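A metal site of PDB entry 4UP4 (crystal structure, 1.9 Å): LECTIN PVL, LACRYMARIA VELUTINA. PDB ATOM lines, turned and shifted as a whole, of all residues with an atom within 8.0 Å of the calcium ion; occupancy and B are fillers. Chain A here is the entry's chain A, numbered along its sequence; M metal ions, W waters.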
ATOM      1  N   ASP A 177     -15.335 -19.365  17.609  1.00  0.00           N
ATOM      2  CA  ASP A 177     -13.975 -19.343  17.149  1.00  0.00           C
ATOM      3  C   ASP A 177     -13.241 -18.206  17.889  1.00  0.00           C
ATOM      4  O   ASP A 177     -13.522 -17.042  17.588  1.00  0.00           O
ATOM      5  CB  ASP A 177     -13.919 -19.062  15.642  1.00  0.00           C
ATOM      6  CG  ASP A 177     -12.474 -19.065  15.076  1.00  0.00           C
ATOM      7  OD1 ASP A 177     -11.506 -19.383  15.818  1.00  0.00           O
ATOM      8  OD2 ASP A 177     -12.320 -18.786  13.890  1.00  0.00           O
ATOM      9  N   ALA A 232     -18.947 -12.577  21.457  1.00  0.00           N
ATOM     10  CA  ALA A 232     -19.207 -11.963  20.216  1.00  0.00           C
ATOM     11  C   ALA A 232     -18.011 -11.158  19.725  1.00  0.00           C
ATOM     12  O   ALA A 232     -17.205 -10.691  20.529  1.00  0.00           O
ATOM     13  CB  ALA A 232     -20.375 -11.002  20.365  1.00  0.00           C
ATOM     14  N   ASP A 233     -17.943 -10.969  18.406  1.00  0.00           N
ATOM     15  CA  ASP A 233     -16.794 -10.243  17.793  1.00  0.00           C
ATOM     16  C   ASP A 233     -17.085  -8.790  17.973  1.00  0.00           C
ATOM     17  O   ASP A 233     -18.045  -8.274  17.412  1.00  0.00           O
ATOM     18  CB  ASP A 233     -16.574 -10.605  16.350  1.00  0.00           C
ATOM     19  CG  ASP A 233     -15.489  -9.772  15.706  1.00  0.00           C
ATOM     20  OD1 ASP A 233     -14.711  -9.141  16.454  1.00  0.00           O
ATOM     21  OD2 ASP A 233     -15.348  -9.832  14.457  1.00  0.00           O
ATOM     22  N   LEU A 234     -16.271  -8.132  18.794  1.00  0.00           N
ATOM     23  CA  LEU A 234     -16.449  -6.699  19.061  1.00  0.00           C
ATOM     24  C   LEU A 234     -15.523  -5.806  18.260  1.00  0.00           C
ATOM     25  O   LEU A 234     -15.638  -4.582  18.325  1.00  0.00           O
ATOM     26  CB  LEU A 234     -16.183  -6.421  20.543  1.00  0.00           C
ATOM     27  CG  LEU A 234     -17.166  -7.133  21.479  1.00  0.00           C
ATOM     28  CD1 LEU A 234     -16.853  -6.785  22.919  1.00  0.00           C
ATOM     29  CD2 LEU A 234     -18.574  -6.774  21.128  1.00  0.00           C
ATOM     30  N   THR A 235     -14.626  -6.401  17.480  1.00  0.00           N
ATOM     31  CA  THR A 235     -13.602  -5.647  16.779  1.00  0.00           C
ATOM     32  C   THR A 235     -13.629  -5.788  15.240  1.00  0.00           C
ATOM     33  O   THR A 235     -13.024  -4.984  14.541  1.00  0.00           O
ATOM     34  CB  THR A 235     -12.196  -6.003  17.266  1.00  0.00           C
ATOM     35  OG1 THR A 235     -11.956  -7.384  17.046  1.00  0.00           O
ATOM     36  CG2 THR A 235     -12.008  -5.752  18.790  1.00  0.00           C
ATOM     37  N   GLY A 236     -14.274  -6.822  14.702  1.00  0.00           N
ATOM     38  CA  GLY A 236     -14.290  -6.986  13.266  1.00  0.00           C
ATOM     39  C   GLY A 236     -13.262  -7.956  12.719  1.00  0.00           C
ATOM     40  O   GLY A 236     -13.248  -8.201  11.527  1.00  0.00           O
ATOM     41  N   ASP A 237     -12.442  -8.597  13.542  1.00  0.00           N
ATOM     42  CA  ASP A 237     -11.506  -9.569  12.991  1.00  0.00           C
ATOM     43  C   ASP A 237     -12.019 -11.004  13.000  1.00  0.00           C
ATOM     44  O   ASP A 237     -11.231 -11.914  12.793  1.00  0.00           O
ATOM     45  CB  ASP A 237     -10.176  -9.530  13.727  1.00  0.00           C
ATOM     46  CG  ASP A 237     -10.291  -9.957  15.153  1.00  0.00           C
ATOM     47  OD1 ASP A 237     -11.429 -10.225  15.629  1.00  0.00           O
ATOM     48  OD2 ASP A 237      -9.234 -10.044  15.831  1.00  0.00           O
ATOM     49  N   ARG A 238     -13.302 -11.198  13.258  1.00  0.00           N
ATOM     50  CA  ARG A 238     -13.905 -12.561  13.285  1.00  0.00           C
ATOM     51  C   ARG A 238     -13.420 -13.472  14.414  1.00  0.00           C
ATOM     52  O   ARG A 238     -13.748 -14.688  14.424  1.00  0.00           O
ATOM     53  CB  ARG A 238     -13.734 -13.260  11.930  1.00  0.00           C
ATOM     54  CG  ARG A 238     -14.137 -12.426  10.734  1.00  0.00           C
ATOM     55  CD  ARG A 238     -14.037 -13.183   9.405  1.00  0.00           C
ATOM     56  NE  ARG A 238     -15.391 -13.618   9.025  1.00  0.00           N
ATOM     57  CZ  ARG A 238     -16.336 -12.762   8.606  1.00  0.00           C
ATOM     58  NH1 ARG A 238     -16.069 -11.456   8.489  1.00  0.00           N
ATOM     59  NH2 ARG A 238     -17.555 -13.198   8.302  1.00  0.00           N
ATOM     60  N   LYS A 239     -12.689 -12.904  15.368  1.00  0.00           N
ATOM     61  CA  LYS A 239     -12.275 -13.609  16.585  1.00  0.00           C
ATOM     62  C   LYS A 239     -13.169 -13.148  17.747  1.00  0.00           C
ATOM     63  O   LYS A 239     -13.387 -11.978  17.945  1.00  0.00           O
ATOM     64  CB  LYS A 239     -10.810 -13.345  16.870  1.00  0.00           C
ATOM     65  CG  LYS A 239      -9.890 -13.914  15.797  1.00  0.00           C
ATOM     66  CD  LYS A 239      -8.460 -13.434  15.902  1.00  0.00           C
ATOM     67  CE  LYS A 239      -7.670 -13.751  14.646  1.00  0.00           C
ATOM     68  NZ  LYS A 239      -6.264 -13.408  14.832  1.00  0.00           N
ATOM     69  N   ALA A 240     -13.789 -14.095  18.464  1.00  0.00           N
ATOM     70  CA  ALA A 240     -14.735 -13.727  19.464  1.00  0.00           C
ATOM     71  C   ALA A 240     -14.059 -13.048  20.701  1.00  0.00           C
ATOM     72  O   ALA A 240     -12.973 -13.477  21.187  1.00  0.00           O
ATOM     73  CB  ALA A 240     -15.564 -14.957  19.883  1.00  0.00           C
ATOM     74  N   ASP A 241     -14.725 -12.003  21.147  1.00  0.00           N
ATOM     75  CA  ASP A 241     -14.471 -11.304  22.406  1.00  0.00           C
ATOM     76  C   ASP A 241     -15.517 -11.641  23.465  1.00  0.00           C
ATOM     77  O   ASP A 241     -16.486 -12.288  23.192  1.00  0.00           O
ATOM     78  CB  ASP A 241     -14.404  -9.803  22.131  1.00  0.00           C
ATOM     79  CG  ASP A 241     -13.476  -9.508  20.966  1.00  0.00           C
ATOM     80  OD1 ASP A 241     -12.261  -9.702  21.157  1.00  0.00           O
ATOM     81  OD2 ASP A 241     -13.943  -9.161  19.834  1.00  0.00           O
ATOM     82  N   ILE A 242     -15.276 -11.158  24.676  1.00  0.00           N
ATOM     83  CA  ILE A 242     -16.164 -11.365  25.809  1.00  0.00           C
ATOM     84  C   ILE A 242     -16.834 -10.065  26.197  1.00  0.00           C
ATOM     85  O   ILE A 242     -16.183  -8.983  26.303  1.00  0.00           O
ATOM     86  CB  ILE A 242     -15.402 -11.993  27.019  1.00  0.00           C
ATOM     87  CG1 ILE A 242     -14.940 -13.395  26.661  1.00  0.00           C
ATOM     88  CG2 ILE A 242     -16.291 -12.106  28.266  1.00  0.00           C
ATOM     89  CD1 ILE A 242     -13.795 -13.937  27.516  1.00  0.00           C
ATOM     90  N   SER A 253     -13.653  -8.127  27.716  1.00  0.00           N
ATOM     91  CA  SER A 253     -12.274  -8.586  27.561  1.00  0.00           C
ATOM     92  C   SER A 253     -12.083  -8.864  26.090  1.00  0.00           C
ATOM     93  O   SER A 253     -12.718  -9.762  25.550  1.00  0.00           O
ATOM     94  CB  SER A 253     -11.982  -9.849  28.396  1.00  0.00           C
ATOM     95  OG  SER A 253     -10.684 -10.352  28.186  1.00  0.00           O
ATOM     96  N   LEU A 254     -11.179  -8.107  25.449  1.00  0.00           N
ATOM     97  CA  LEU A 254     -10.848  -8.350  24.062  1.00  0.00           C
ATOM     98  C   LEU A 254      -9.820  -9.428  23.828  1.00  0.00           C
ATOM     99  O   LEU A 254      -8.785  -9.535  24.518  1.00  0.00           O
ATOM    100  CB  LEU A 254     -10.416  -7.030  23.357  1.00  0.00           C
ATOM    101  CG  LEU A 254     -11.414  -5.889  23.508  1.00  0.00           C
ATOM    102  CD1 LEU A 254     -10.921  -4.631  22.812  1.00  0.00           C
ATOM    103  CD2 LEU A 254     -12.813  -6.239  22.992  1.00  0.00           C
ATOM    104  N   ASN A 255     -10.116 -10.269  22.825  1.00  0.00           N
ATOM    105  CA  ASN A 255      -9.182 -11.295  22.298  1.00  0.00           C
ATOM    106  C   ASN A 255      -7.897 -10.579  21.892  1.00  0.00           C
ATOM    107  O   ASN A 255      -7.940  -9.571  21.180  1.00  0.00           O
ATOM    108  CB  ASN A 255      -9.804 -12.004  21.086  1.00  0.00           C
ATOM    109  CG  ASN A 255      -9.229 -13.390  20.815  1.00  0.00           C
ATOM    110  OD1 ASN A 255      -8.025 -13.547  20.598  1.00  0.00           O
ATOM    111  ND2 ASN A 255     -10.108 -14.415  20.755  1.00  0.00           N
ATOM    112  N   ASN A 256      -6.766 -11.113  22.358  1.00  0.00           N
ATOM    113  CA  ASN A 256      -5.458 -10.618  21.940  1.00  0.00           C
ATOM    114  C   ASN A 256      -5.196 -11.021  20.488  1.00  0.00           C
ATOM    115  O   ASN A 256      -4.323 -10.452  19.823  1.00  0.00           O
ATOM    116  CB  ASN A 256      -4.345 -11.191  22.837  1.00  0.00           C
ATOM    117  CG  ASN A 256      -4.342 -10.583  24.232  1.00  0.00           C
ATOM    118  OD1 ASN A 256      -4.121 -11.293  25.218  1.00  0.00           O
ATOM    119  ND2 ASN A 256      -4.621  -9.307  24.342  1.00  0.00           N
ATOM    120  N   GLY A 257      -5.910 -12.039  19.999  1.00  0.00           N
ATOM    121  CA  GLY A 257      -5.750 -12.437  18.607  1.00  0.00           C
ATOM    122  C   GLY A 257      -5.371 -13.892  18.461  1.00  0.00           C
ATOM    123  O   GLY A 257      -5.435 -14.435  17.394  1.00  0.00           O
ATOM    124  N   PHE A 261      -6.671 -13.438  26.123  1.00  0.00           N
ATOM    125  CA  PHE A 261      -7.585 -12.342  26.322  1.00  0.00           C
ATOM    126  C   PHE A 261      -6.978 -11.257  27.190  1.00  0.00           C
ATOM    127  O   PHE A 261      -6.204 -11.530  28.094  1.00  0.00           O
ATOM    128  CB  PHE A 261      -8.848 -12.885  26.956  1.00  0.00           C
ATOM    129  CG  PHE A 261      -9.740 -13.594  25.981  1.00  0.00           C
ATOM    130  CD1 PHE A 261      -9.501 -14.911  25.649  1.00  0.00           C
ATOM    131  CD2 PHE A 261     -10.787 -12.921  25.330  1.00  0.00           C
ATOM    132  CE1 PHE A 261     -10.296 -15.565  24.719  1.00  0.00           C
ATOM    133  CE2 PHE A 261     -11.576 -13.569  24.384  1.00  0.00           C
ATOM    134  CZ  PHE A 261     -11.325 -14.891  24.068  1.00  0.00           C
ATOM    135  N   VAL A 294     -19.803  -5.417  13.553  1.00  0.00           N
ATOM    136  CA  VAL A 294     -19.251  -5.694  14.893  1.00  0.00           C
ATOM    137  C   VAL A 294     -20.407  -5.733  15.890  1.00  0.00           C
ATOM    138  O   VAL A 294     -21.515  -5.330  15.574  1.00  0.00           O
ATOM    139  CB  VAL A 294     -18.258  -4.607  15.349  1.00  0.00           C
ATOM    140  CG1 VAL A 294     -16.979  -4.694  14.544  1.00  0.00           C
ATOM    141  CG2 VAL A 294     -18.880  -3.211  15.260  1.00  0.00           C
ATOM    142  N   GLY A 312     -16.183   0.434  16.453  1.00  0.00           N
ATOM    143  CA  GLY A 312     -15.489  -0.453  15.541  1.00  0.00           C
ATOM    144  C   GLY A 312     -14.405  -1.246  16.255  1.00  0.00           C
ATOM    145  O   GLY A 312     -13.893  -2.265  15.744  1.00  0.00           O
HETATM  146 CA    CA M   1     -12.704  -9.655  17.679  1.00  0.00          CA
HETATM  147  O   HOH W   1     -10.591  -9.054  19.203  1.00  0.00           O
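Water W1 lies within hydrogen-bond range of OD1 of Asp 241 and O of Asn 255.
NZ of Lys 239 lies within hydrogen-bond range of O of Gly 257 (2.9 Å). N of Asp 241 sits at hydrogen-bond distance from O of Ala 232. The backbone NH (N) of Arg 238 sits at hydrogen-bond distance from the side-chain carboxylate (OD2) of Asp 233 (2.7 Å). OD1 of Asp 241 lies within hydrogen-bond range of N of Asn 255, 2.8 Å away. OD2 of Asp 241 sits close to N of Leu 234, 2.7 Å away. OD2 of Asp 233 is in hydrogen-bond range of N of Gly 236 (3.2 Å).
The calcium ion is bound by the side-chain carboxylate (OD1) of Asp 233 (2.4 Å). The calcium ion is bound by the backbone carbonyl oxygen (O) of Lys 239 (2.4 Å). OG1 of Thr 235 binds the calcium ion. The calcium ion is bound by OD1 of Asp 237, at 2.5 Å. The side-chain carboxylate (OD2) of Asp 241 is bound to the calcium ion, 2.5 Å away. Water W1 binds the calcium ion (2.7 Å).
Five residues have an atom within 4 Å of the calcium ion: Asp 233, Thr 235, Asp 237, Lys 239 and Asp 241.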
